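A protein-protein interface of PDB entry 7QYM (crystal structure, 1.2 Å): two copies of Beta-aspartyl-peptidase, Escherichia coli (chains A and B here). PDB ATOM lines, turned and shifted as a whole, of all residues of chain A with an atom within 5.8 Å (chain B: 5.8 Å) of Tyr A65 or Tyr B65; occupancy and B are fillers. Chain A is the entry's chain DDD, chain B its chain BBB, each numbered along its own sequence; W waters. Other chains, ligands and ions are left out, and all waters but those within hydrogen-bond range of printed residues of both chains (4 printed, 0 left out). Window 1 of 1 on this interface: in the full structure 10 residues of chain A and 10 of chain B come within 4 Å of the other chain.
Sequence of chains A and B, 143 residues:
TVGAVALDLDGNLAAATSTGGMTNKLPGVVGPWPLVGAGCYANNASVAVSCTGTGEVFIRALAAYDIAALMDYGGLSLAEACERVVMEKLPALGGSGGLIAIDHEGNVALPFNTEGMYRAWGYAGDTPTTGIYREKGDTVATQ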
ATOM      1  N   GLY A  37       4.695 -22.469 -14.297  1.00  0.00           N
ATOM      2  CA  GLY A  37       5.944 -21.701 -14.241  1.00  0.00           C
ATOM      3  C   GLY A  37       7.088 -22.325 -14.981  1.00  0.00           C
ATOM      4  O   GLY A  37       8.064 -21.616 -15.261  1.00  0.00           O
ATOM      5  N   ALA A  38       7.021 -23.616 -15.242  1.00  0.00           N
ATOM      6  CA  ALA A  38       8.075 -24.324 -15.970  1.00  0.00           C
ATOM      7  C   ALA A  38       7.648 -24.495 -17.412  1.00  0.00           C
ATOM      8  O   ALA A  38       8.312 -23.942 -18.293  1.00  0.00           O
ATOM      9  CB  ALA A  38       8.440 -25.618 -15.305  1.00  0.00           C
ATOM     10  N   TYR A  41       2.603 -20.885 -18.274  1.00  0.00           N
ATOM     11  CA  TYR A  41       2.358 -19.762 -17.351  1.00  0.00           C
ATOM     12  C   TYR A  41       1.558 -18.719 -18.095  1.00  0.00           C
ATOM     13  O   TYR A  41       1.784 -18.505 -19.276  1.00  0.00           O
ATOM     14  CB  TYR A  41       3.666 -19.158 -16.862  1.00  0.00           C
ATOM     15  CG  TYR A  41       3.473 -18.075 -15.832  1.00  0.00           C
ATOM     16  CD1 TYR A  41       3.061 -18.369 -14.544  1.00  0.00           C
ATOM     17  CD2 TYR A  41       3.626 -16.737 -16.164  1.00  0.00           C
ATOM     18  CE1 TYR A  41       2.765 -17.385 -13.615  1.00  0.00           C
ATOM     19  CE2 TYR A  41       3.327 -15.733 -15.252  1.00  0.00           C
ATOM     20  CZ  TYR A  41       2.917 -16.054 -13.961  1.00  0.00           C
ATOM     21  OH  TYR A  41       2.607 -15.064 -13.064  1.00  0.00           O
ATOM     22  N   ASN A  43      -0.144 -14.602 -17.216  1.00  0.00           N
ATOM     23  CA  ASN A  43      -0.458 -13.494 -16.300  1.00  0.00           C
ATOM     24  C   ASN A  43      -0.731 -12.271 -17.164  1.00  0.00           C
ATOM     25  O   ASN A  43       0.128 -11.840 -17.948  1.00  0.00           O
ATOM     26  CB  ASN A  43       0.701 -13.264 -15.362  1.00  0.00           C
ATOM     27  CG  ASN A  43       0.431 -12.274 -14.267  1.00  0.00           C
ATOM     28  OD1 ASN A  43      -0.320 -11.306 -14.458  1.00  0.00           O
ATOM     29  ND2 ASN A  43       1.016 -12.542 -13.111  1.00  0.00           N
ATOM     30  N   ARG A  60      14.376 -26.536 -13.801  1.00  0.00           N
ATOM     31  CA  ARG A  60      15.440 -25.933 -12.964  1.00  0.00           C
ATOM     32  C   ARG A  60      15.533 -24.426 -13.180  1.00  0.00           C
ATOM     33  O   ARG A  60      15.877 -23.720 -12.215  1.00  0.00           O
ATOM     34  CB  ARG A  60      16.765 -26.583 -13.328  1.00  0.00           C
ATOM     35  CG  ARG A  60      16.833 -28.054 -12.944  1.00  0.00           C
ATOM     36  CD  ARG A  60      17.987 -28.797 -13.608  1.00  0.00           C
ATOM     37  NE  ARG A  60      19.257 -28.224 -13.266  1.00  0.00           N
ATOM     38  CZ  ARG A  60      20.363 -28.384 -13.966  1.00  0.00           C
ATOM     39  NH1 ARG A  60      20.343 -29.121 -15.065  1.00  0.00           N
ATOM     40  NH2 ARG A  60      21.495 -27.833 -13.550  1.00  0.00           N
ATOM     41  N   ALA A  61      15.275 -23.991 -14.410  1.00  0.00           N
ATOM     42  CA  ALA A  61      15.358 -22.575 -14.778  1.00  0.00           C
ATOM     43  C   ALA A  61      14.009 -21.882 -14.754  1.00  0.00           C
ATOM     44  O   ALA A  61      13.913 -20.717 -15.085  1.00  0.00           O
ATOM     45  CB  ALA A  61      15.966 -22.448 -16.139  1.00  0.00           C
ATOM     46  N   LEU A  62      12.937 -22.596 -14.403  1.00  0.00           N
ATOM     47  CA  LEU A  62      11.534 -22.115 -14.372  1.00  0.00           C
ATOM     48  C   LEU A  62      11.307 -21.215 -15.587  1.00  0.00           C
ATOM     49  O   LEU A  62      10.920 -20.044 -15.464  1.00  0.00           O
ATOM     50  CB  LEU A  62      11.249 -21.450 -13.026  1.00  0.00           C
ATOM     51  CG  LEU A  62       9.811 -21.535 -12.550  1.00  0.00           C
ATOM     52  CD1 LEU A  62       9.367 -22.964 -12.248  1.00  0.00           C
ATOM     53  CD2 LEU A  62       9.619 -20.650 -11.326  1.00  0.00           C
ATOM     54  N   ALA A  63      11.455 -21.796 -16.757  1.00  0.00           N
ATOM     55  CA  ALA A  63      11.596 -21.015 -17.995  1.00  0.00           C
ATOM     56  C   ALA A  63      10.385 -20.135 -18.260  1.00  0.00           C
ATOM     57  O   ALA A  63      10.540 -18.975 -18.644  1.00  0.00           O
ATOM     58  CB  ALA A  63      11.845 -21.913 -19.173  1.00  0.00           C
ATOM     59  N   ALA A  64       9.159 -20.675 -18.127  1.00  0.00           N
ATOM     60  CA  ALA A  64       7.976 -19.900 -18.480  1.00  0.00           C
ATOM     61  C   ALA A  64       7.842 -18.685 -17.554  1.00  0.00           C
ATOM     62  O   ALA A  64       7.559 -17.560 -18.026  1.00  0.00           O
ATOM     63  CB  ALA A  64       6.747 -20.781 -18.451  1.00  0.00           C
ATOM     64  N   TYR A  65       7.947 -18.889 -16.249  1.00  0.00           N
ATOM     65  CA  TYR A  65       7.871 -17.755 -15.313  1.00  0.00           C
ATOM     66  C   TYR A  65       9.052 -16.814 -15.496  1.00  0.00           C
ATOM     67  O   TYR A  65       8.878 -15.628 -15.301  1.00  0.00           O
ATOM     68  CB  TYR A  65       7.777 -18.224 -13.867  1.00  0.00           C
ATOM     69  CG  TYR A  65       7.414 -17.136 -12.914  1.00  0.00           C
ATOM     70  CD1 TYR A  65       6.153 -16.624 -12.871  1.00  0.00           C
ATOM     71  CD2 TYR A  65       8.324 -16.538 -12.111  1.00  0.00           C
ATOM     72  CE1 TYR A  65       5.812 -15.581 -12.040  1.00  0.00           C
ATOM     73  CE2 TYR A  65       8.019 -15.489 -11.273  1.00  0.00           C
ATOM     74  CZ  TYR A  65       6.741 -15.014 -11.211  1.00  0.00           C
ATOM     75  OH  TYR A  65       6.410 -13.964 -10.391  1.00  0.00           O
ATOM     76  N   ASP A  66      10.214 -17.335 -15.834  1.00  0.00           N
ATOM     77  CA  ASP A  66      11.402 -16.471 -15.985  1.00  0.00           C
ATOM     78  C   ASP A  66      11.128 -15.443 -17.102  1.00  0.00           C
ATOM     79  O   ASP A  66      11.531 -14.285 -16.946  1.00  0.00           O
ATOM     80  CB  ASP A  66      12.651 -17.304 -16.255  1.00  0.00           C
ATOM     81  CG  ASP A  66      13.928 -16.574 -15.923  1.00  0.00           C
ATOM     82  OD1 ASP A  66      13.893 -15.830 -14.902  1.00  0.00           O
ATOM     83  OD2 ASP A  66      14.894 -16.756 -16.638  1.00  0.00           O
ATOM     84  N   ILE A  67      10.494 -15.837 -18.201  1.00  0.00           N
ATOM     85  CA  ILE A  67      10.115 -14.870 -19.267  1.00  0.00           C
ATOM     86  C   ILE A  67       9.321 -13.739 -18.593  1.00  0.00           C
ATOM     87  O   ILE A  67       9.589 -12.544 -18.806  1.00  0.00           O
ATOM     88  CB  ILE A  67       9.308 -15.534 -20.391  1.00  0.00           C
ATOM     89  CG1 ILE A  67      10.097 -16.636 -21.116  1.00  0.00           C
ATOM     90  CG2 ILE A  67       8.815 -14.458 -21.339  1.00  0.00           C
ATOM     91  CD1 ILE A  67      11.139 -16.093 -21.998  1.00  0.00           C
ATOM     92  N   ALA A  68       8.276 -14.129 -17.880  1.00  0.00           N
ATOM     93  CA  ALA A  68       7.373 -13.176 -17.231  1.00  0.00           C
ATOM     94  C   ALA A  68       8.137 -12.242 -16.294  1.00  0.00           C
ATOM     95  O   ALA A  68       7.906 -11.050 -16.299  1.00  0.00           O
ATOM     96  CB  ALA A  68       6.268 -13.883 -16.473  1.00  0.00           C
ATOM     97  N   ALA A  69       9.003 -12.791 -15.468  1.00  0.00           N
ATOM     98  CA  ALA A  69       9.712 -12.008 -14.427  1.00  0.00           C
ATOM     99  C   ALA A  69      10.741 -11.103 -15.081  1.00  0.00           C
ATOM    100  O   ALA A  69      10.897  -9.943 -14.647  1.00  0.00           O
ATOM    101  CB  ALA A  69      10.348 -12.932 -13.431  1.00  0.00           C
ATOM    102  N   LEU A  70      11.395 -11.565 -16.135  1.00  0.00           N
ATOM    103  CA  LEU A  70      12.353 -10.717 -16.859  1.00  0.00           C
ATOM    104  C   LEU A  70      11.619  -9.495 -17.451  1.00  0.00           C
ATOM    105  O   LEU A  70      12.169  -8.389 -17.422  1.00  0.00           O
ATOM    106  CB  LEU A  70      13.040 -11.540 -17.936  1.00  0.00           C
ATOM    107  CG  LEU A  70      14.160 -12.443 -17.460  1.00  0.00           C
ATOM    108  CD1 LEU A  70      14.524 -13.431 -18.561  1.00  0.00           C
ATOM    109  CD2 LEU A  70      15.361 -11.618 -17.028  1.00  0.00           C
ATOM    110  N   TYR A  73       9.717  -7.487 -13.963  1.00  0.00           N
ATOM    111  CA  TYR A  73      10.668  -6.943 -12.971  1.00  0.00           C
ATOM    112  C   TYR A  73      11.907  -6.375 -13.643  1.00  0.00           C
ATOM    113  O   TYR A  73      12.432  -5.363 -13.157  1.00  0.00           O
ATOM    114  CB  TYR A  73      11.125  -8.030 -12.005  1.00  0.00           C
ATOM    115  CG  TYR A  73      10.002  -8.730 -11.286  1.00  0.00           C
ATOM    116  CD1 TYR A  73       8.757  -8.155 -11.074  1.00  0.00           C
ATOM    117  CD2 TYR A  73      10.218  -9.994 -10.777  1.00  0.00           C
ATOM    118  CE1 TYR A  73       7.755  -8.821 -10.395  1.00  0.00           C
ATOM    119  CE2 TYR A  73       9.235 -10.677 -10.083  1.00  0.00           C
ATOM    120  CZ  TYR A  73       7.995 -10.098  -9.911  1.00  0.00           C
ATOM    121  OH  TYR A  73       7.015 -10.757  -9.252  1.00  0.00           O
ATOM    122  N   LYS A  89      20.284 -18.742 -21.353  1.00  0.00           N
ATOM    123  CA  LYS A  89      20.208 -19.431 -20.044  1.00  0.00           C
ATOM    124  C   LYS A  89      19.978 -20.920 -20.247  1.00  0.00           C
ATOM    125  O   LYS A  89      20.604 -21.742 -19.569  1.00  0.00           O
ATOM    126  CB  LYS A  89      19.132 -18.806 -19.167  1.00  0.00           C
ATOM    127  CG  LYS A  89      19.441 -17.373 -18.758  1.00  0.00           C
ATOM    128  CD  LYS A  89      18.348 -16.749 -17.934  1.00  0.00           C
ATOM    129  CE  LYS A  89      18.329 -17.278 -16.523  1.00  0.00           C
ATOM    130  NZ  LYS A  89      17.434 -16.449 -15.681  1.00  0.00           N
ATOM    131  N   GLY B  37      10.530 -24.015  -7.459  1.00  0.00           N
ATOM    132  CA  GLY B  37      10.065 -22.652  -7.688  1.00  0.00           C
ATOM    133  C   GLY B  37       8.804 -22.309  -6.957  1.00  0.00           C
ATOM    134  O   GLY B  37       8.516 -21.109  -6.821  1.00  0.00           O
ATOM    135  N   ALA B  38       8.015 -23.289  -6.529  1.00  0.00           N
ATOM    136  CA  ALA B  38       6.776 -23.026  -5.794  1.00  0.00           C
ATOM    137  C   ALA B  38       7.077 -23.229  -4.319  1.00  0.00           C
ATOM    138  O   ALA B  38       7.007 -22.239  -3.615  1.00  0.00           O
ATOM    139  CB  ALA B  38       5.656 -23.894  -6.285  1.00  0.00           C
ATOM    140  N   TYR B  41      13.284 -23.539  -3.606  1.00  0.00           N
ATOM    141  CA  TYR B  41      14.154 -23.012  -4.666  1.00  0.00           C
ATOM    142  C   TYR B  41      15.484 -22.623  -4.047  1.00  0.00           C
ATOM    143  O   TYR B  41      15.507 -22.154  -2.936  1.00  0.00           O
ATOM    144  CB  TYR B  41      13.545 -21.787  -5.350  1.00  0.00           C
ATOM    145  CG  TYR B  41      14.354 -21.260  -6.503  1.00  0.00           C
ATOM    146  CD1 TYR B  41      14.411 -21.925  -7.700  1.00  0.00           C
ATOM    147  CD2 TYR B  41      15.146 -20.120  -6.367  1.00  0.00           C
ATOM    148  CE1 TYR B  41      15.222 -21.515  -8.733  1.00  0.00           C
ATOM    149  CE2 TYR B  41      15.960 -19.686  -7.390  1.00  0.00           C
ATOM    150  CZ  TYR B  41      16.005 -20.382  -8.580  1.00  0.00           C
ATOM    151  OH  TYR B  41      16.801 -19.948  -9.606  1.00  0.00           O
ATOM    152  N   ARG B  60       0.407 -20.983  -7.860  1.00  0.00           N
ATOM    153  CA  ARG B  60      -0.048 -19.942  -8.806  1.00  0.00           C
ATOM    154  C   ARG B  60       0.924 -18.748  -8.803  1.00  0.00           C
ATOM    155  O   ARG B  60       1.109 -18.124  -9.863  1.00  0.00           O
ATOM    156  CB  ARG B  60      -1.451 -19.517  -8.445  1.00  0.00           C
ATOM    157  CG  ARG B  60      -2.460 -20.629  -8.698  1.00  0.00           C
ATOM    158  CD  ARG B  60      -3.751 -20.372  -7.937  1.00  0.00           C
ATOM    159  NE  ARG B  60      -4.371 -19.141  -8.395  1.00  0.00           N
ATOM    160  CZ  ARG B  60      -5.362 -18.514  -7.797  1.00  0.00           C
ATOM    161  NH1 ARG B  60      -5.827 -18.908  -6.631  1.00  0.00           N
ATOM    162  NH2 ARG B  60      -5.896 -17.432  -8.315  1.00  0.00           N
ATOM    163  N   ALA B  61       1.434 -18.425  -7.623  1.00  0.00           N
ATOM    164  CA  ALA B  61       2.320 -17.272  -7.396  1.00  0.00           C
ATOM    165  C   ALA B  61       3.798 -17.632  -7.566  1.00  0.00           C
ATOM    166  O   ALA B  61       4.640 -16.733  -7.441  1.00  0.00           O
ATOM    167  CB  ALA B  61       2.035 -16.712  -6.017  1.00  0.00           C
ATOM    168  N   LEU B  62       4.124 -18.893  -7.811  1.00  0.00           N
ATOM    169  CA  LEU B  62       5.523 -19.376  -7.917  1.00  0.00           C
ATOM    170  C   LEU B  62       6.326 -18.729  -6.791  1.00  0.00           C
ATOM    171  O   LEU B  62       7.351 -18.129  -7.078  1.00  0.00           O
ATOM    172  CB  LEU B  62       6.129 -19.040  -9.282  1.00  0.00           C
ATOM    173  CG  LEU B  62       5.727 -19.938 -10.450  1.00  0.00           C
ATOM    174  CD1 LEU B  62       5.572 -21.406 -10.045  1.00  0.00           C
ATOM    175  CD2 LEU B  62       4.483 -19.445 -11.114  1.00  0.00           C
ATOM    176  N   ALA B  63       5.912 -18.881  -5.554  1.00  0.00           N
ATOM    177  CA  ALA B  63       6.345 -17.991  -4.465  1.00  0.00           C
ATOM    178  C   ALA B  63       7.849 -18.059  -4.249  1.00  0.00           C
ATOM    179  O   ALA B  63       8.494 -17.024  -4.070  1.00  0.00           O
ATOM    180  CB  ALA B  63       5.627 -18.355  -3.200  1.00  0.00           C
ATOM    181  N   ALA B  64       8.427 -19.266  -4.233  1.00  0.00           N
ATOM    182  CA  ALA B  64       9.860 -19.403  -3.907  1.00  0.00           C
ATOM    183  C   ALA B  64      10.712 -18.721  -5.003  1.00  0.00           C
ATOM    184  O   ALA B  64      11.661 -17.967  -4.680  1.00  0.00           O
ATOM    185  CB  ALA B  64      10.232 -20.868  -3.748  1.00  0.00           C
ATOM    186  N   TYR B  65      10.420 -18.993  -6.266  1.00  0.00           N
ATOM    187  CA  TYR B  65      11.181 -18.353  -7.363  1.00  0.00           C
ATOM    188  C   TYR B  65      10.866 -16.860  -7.412  1.00  0.00           C
ATOM    189  O   TYR B  65      11.737 -16.083  -7.748  1.00  0.00           O
ATOM    190  CB  TYR B  65      10.870 -18.977  -8.719  1.00  0.00           C
ATOM    191  CG  TYR B  65      11.778 -18.497  -9.809  1.00  0.00           C
ATOM    192  CD1 TYR B  65      13.068 -18.932  -9.870  1.00  0.00           C
ATOM    193  CD2 TYR B  65      11.406 -17.550 -10.716  1.00  0.00           C
ATOM    194  CE1 TYR B  65      13.918 -18.522 -10.862  1.00  0.00           C
ATOM    195  CE2 TYR B  65      12.241 -17.130 -11.718  1.00  0.00           C
ATOM    196  CZ  TYR B  65      13.511 -17.584 -11.771  1.00  0.00           C
ATOM    197  OH  TYR B  65      14.400 -17.155 -12.686  1.00  0.00           O
ATOM    198  N   ASP B  66       9.654 -16.464  -7.060  1.00  0.00           N
ATOM    199  CA  ASP B  66       9.297 -15.029  -7.105  1.00  0.00           C
ATOM    200  C   ASP B  66      10.181 -14.239  -6.134  1.00  0.00           C
ATOM    201  O   ASP B  66      10.599 -13.122  -6.499  1.00  0.00           O
ATOM    202  CB  ASP B  66       7.821 -14.833  -6.796  1.00  0.00           C
ATOM    203  CG  ASP B  66       7.302 -13.495  -7.305  1.00  0.00           C
ATOM    204  OD1 ASP B  66       7.752 -13.100  -8.400  1.00  0.00           O
ATOM    205  OD2 ASP B  66       6.460 -12.900  -6.642  1.00  0.00           O
ATOM    206  N   ILE B  67      10.506 -14.786  -4.968  1.00  0.00           N
ATOM    207  CA  ILE B  67      11.448 -14.126  -4.038  1.00  0.00           C
ATOM    208  C   ILE B  67      12.751 -13.881  -4.802  1.00  0.00           C
ATOM    209  O   ILE B  67      13.294 -12.745  -4.826  1.00  0.00           O
ATOM    210  CB  ILE B  67      11.710 -14.935  -2.768  1.00  0.00           C
ATOM    211  CG1 ILE B  67      10.442 -15.167  -1.942  1.00  0.00           C
ATOM    212  CG2 ILE B  67      12.820 -14.318  -1.945  1.00  0.00           C
ATOM    213  CD1 ILE B  67       9.941 -13.957  -1.278  1.00  0.00           C
ATOM    214  N   ALA B  68      13.291 -14.931  -5.423  1.00  0.00           N
ATOM    215  CA  ALA B  68      14.546 -14.839  -6.181  1.00  0.00           C
ATOM    216  C   ALA B  68      14.460 -13.788  -7.281  1.00  0.00           C
ATOM    217  O   ALA B  68      15.413 -13.020  -7.448  1.00  0.00           O
ATOM    218  CB  ALA B  68      14.915 -16.185  -6.728  1.00  0.00           C
ATOM    219  N   ALA B  69      13.426 -13.829  -8.080  1.00  0.00           N
ATOM    220  CA  ALA B  69      13.308 -12.904  -9.227  1.00  0.00           C
ATOM    221  C   ALA B  69      13.090 -11.458  -8.784  1.00  0.00           C
ATOM    222  O   ALA B  69      13.686 -10.568  -9.396  1.00  0.00           O
ATOM    223  CB  ALA B  69      12.180 -13.370 -10.092  1.00  0.00           C
ATOM    224  N   LEU B  70      12.345 -11.251  -7.713  1.00  0.00           N
ATOM    225  CA  LEU B  70      12.180  -9.885  -7.182  1.00  0.00           C
ATOM    226  C   LEU B  70      13.537  -9.353  -6.727  1.00  0.00           C
ATOM    227  O   LEU B  70      13.814  -8.153  -6.946  1.00  0.00           O
ATOM    228  CB  LEU B  70      11.185  -9.857  -6.028  1.00  0.00           C
ATOM    229  CG  LEU B  70       9.716  -9.977  -6.431  1.00  0.00           C
ATOM    230  CD1 LEU B  70       8.866 -10.329  -5.222  1.00  0.00           C
ATOM    231  CD2 LEU B  70       9.249  -8.682  -7.075  1.00  0.00           C
ATOM    232  N   TYR B  73      16.089  -9.482 -10.339  1.00  0.00           N
ATOM    233  CA  TYR B  73      15.652  -8.619 -11.458  1.00  0.00           C
ATOM    234  C   TYR B  73      15.068  -7.329 -10.919  1.00  0.00           C
ATOM    235  O   TYR B  73      15.325  -6.297 -11.527  1.00  0.00           O
ATOM    236  CB  TYR B  73      14.605  -9.296 -12.337  1.00  0.00           C
ATOM    237  CG  TYR B  73      15.019 -10.644 -12.865  1.00  0.00           C
ATOM    238  CD1 TYR B  73      16.330 -11.048 -13.057  1.00  0.00           C
ATOM    239  CD2 TYR B  73      14.031 -11.560 -13.184  1.00  0.00           C
ATOM    240  CE1 TYR B  73      16.652 -12.286 -13.576  1.00  0.00           C
ATOM    241  CE2 TYR B  73      14.330 -12.797 -13.723  1.00  0.00           C
ATOM    242  CZ  TYR B  73      15.649 -13.175 -13.900  1.00  0.00           C
ATOM    243  OH  TYR B  73      15.990 -14.390 -14.414  1.00  0.00           O
ATOM    244  N   LYS B  89       1.111 -10.438  -2.026  1.00  0.00           N
ATOM    245  CA  LYS B  89       0.701 -11.226  -3.215  1.00  0.00           C
ATOM    246  C   LYS B  89      -0.093 -12.460  -2.776  1.00  0.00           C
ATOM    247  O   LYS B  89      -1.110 -12.783  -3.396  1.00  0.00           O
ATOM    248  CB  LYS B  89       1.928 -11.511  -4.068  1.00  0.00           C
ATOM    249  CG  LYS B  89       2.651 -10.268  -4.574  1.00  0.00           C
ATOM    250  CD  LYS B  89       3.859 -10.502  -5.445  1.00  0.00           C
ATOM    251  CE  LYS B  89       3.514 -11.029  -6.813  1.00  0.00           C
ATOM    252  NZ  LYS B  89       4.709 -11.041  -7.692  1.00  0.00           N
HETATM  253  O   HOH W   1       3.988 -14.297  -8.893  1.00  0.00           O
HETATM  254  O   HOH W   2       1.709 -15.690 -10.793  1.00  0.00           O
HETATM  255  O   HOH W   3      17.020 -21.328 -11.710  1.00  0.00           O
HETATM  256  O   HOH W   4      16.044 -19.061 -13.966  1.00  0.00           O
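The side-chain carboxylate of Asp A66 is in hydrogen-bond range of the side-chain hydroxyl of Tyr B65, 2.6 Å away.
The side-chain carboxylate of Asp B66 is in hydrogen-bond range of the side-chain hydroxyl of Tyr A65.
The side-chain carboxylate (OD1) of Asp B66 lies within hydrogen-bond range of the side-chain hydroxyl (OH) of Tyr A73.
OD1 of Asp A66 lies within hydrogen-bond range of OH of Tyr B73.
OH of Tyr B73 is in hydrogen-bond range of NZ of Lys A89, 2.8 Å away.
NZ of Lys B89 lies within hydrogen-bond range of OH of Tyr A73 (2.8 Å).
The backbone carbonyl oxygen (O) of Tyr B73 lies close to the backbone carbonyl oxygen (O) of Tyr A73 (3.4 Å).
O of Gly B37 lies within hydrogen-bond range of N of Tyr B65 (2.9 Å).
OD2 of Asp B66 lies within salt-bridge range of NZ of Lys B89, 2.8 Å away.
The backbone NH (N) of Tyr A65 is in hydrogen-bond range of the backbone carbonyl oxygen (O) of Gly A37, 2.9 Å away.
OH of Tyr A41 lies within hydrogen-bond range of ND2 of Asn A43, at 3.0 Å.
OH of Tyr A65 lies within hydrogen-bond range of OH of Tyr A73, 3.5 Å away.
OD2 of Asp A66 lies within salt-bridge range of NZ of Lys A89, 2.7 Å away.
Tyr A41 touches Leu B62.
Tyr B65 touches Leu A62.
Leu B62 touches Tyr A65 (CD2 to CD1, 3.7 Å).
Tyr A65 touches Tyr B65.
Ala A69 touches Ala B69 (CB to CB, 3.8 Å).
Tyr B73 touches Ala A69 (CD2 to O, 3.8 Å).
Tyr B73 touches Leu A70 (CZ to CD2, 3.5 Å).
Tyr A73 touches Ala B69 (CD2 to O, 3.8 Å).
Leu B70 touches Tyr A73 (CD2 to CZ, 3.4 Å).
Ala A64 touches none of the printed residues of chain B.
Of the printed residues of chain B, Tyr A65 touches Leu B62 (3.7 Å), Tyr B65 (3.5 Å) and Asp B66 (2.6 Å).
Printed residues of chain B within 4 Å of Leu A70: Tyr B73.
Tyr B41 touches none of the printed residues of chain A.
Of the printed residues of chain A, Tyr B65 touches Leu A62, Tyr A65 and Asp A66.
Of the printed residues of chain A, Lys B89 touches Tyr A73 (2.8 Å).
The nearest printed residue of chain B that does not touch Tyr A65 is Lys B89 (4.3 Å).
The nearest printed residue of chain A that does not touch Tyr B65 is Lys A89 (4.3 Å).
Of the 16 printed residues of chain B, 7 touch a printed residue of chain A.
Printed residues of chain B that touch a printed residue of chain A: Leu B62, Tyr B65, Asp B66, Ala B69, Leu B70, Tyr B73 and Lys B89.
Hydrophobic or aromatic side chains of chain B within 4 Å of the printed part of chain A: Leu B62, Tyr B65, Ala B69, Leu B70 and Tyr B73.
Hydrophobic or aromatic side chains of chain A within 4 Å of the printed part of chain B: Tyr A41, Leu A62, Tyr A65, Ala A69, Leu A70 and Tyr A73.
Along chain A the printed residues that touch a printed residue of chain B span positions 41 to 89.
Among the printed residues, no Asp or Glu carboxylate lies within 4 Å of a Lys or Arg side-chain nitrogen of the other chain.
Leu A62 touches Tyr B65, and with the chains exchanged Tyr A65 touches Leu B62.
Tyr A65 touches Asp B66, and with the chains exchanged Asp A66 touches Tyr B65.
Leu A70 touches Tyr B73, and with the chains exchanged Tyr A73 touches Leu B70.
Tyr A73 touches Lys B89, and with the chains exchanged Lys A89 touches Tyr B73.
Of the 16 pairs that touch across the chains among the printed residues, 15 have their exchanged pair printed and touching as well.
Water W2 lies within hydrogen-bond range of OH of Tyr A41 and O of Arg B60.
Water W3 bridges the side-chain hydroxyl (OH) of Tyr B41 and the backbone carbonyl oxygen (O) of Arg A60.
Water W4 lies within hydrogen-bond range of the side-chain hydroxyl of Tyr B65 (2.8 Å), the backbone carbonyl oxygen of Ala A61 (2.9 Å) and the side-chain amino group of Lys A89 (3.4 Å).
Water W1 bridges OH of Tyr A65 and O of Ala B61.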
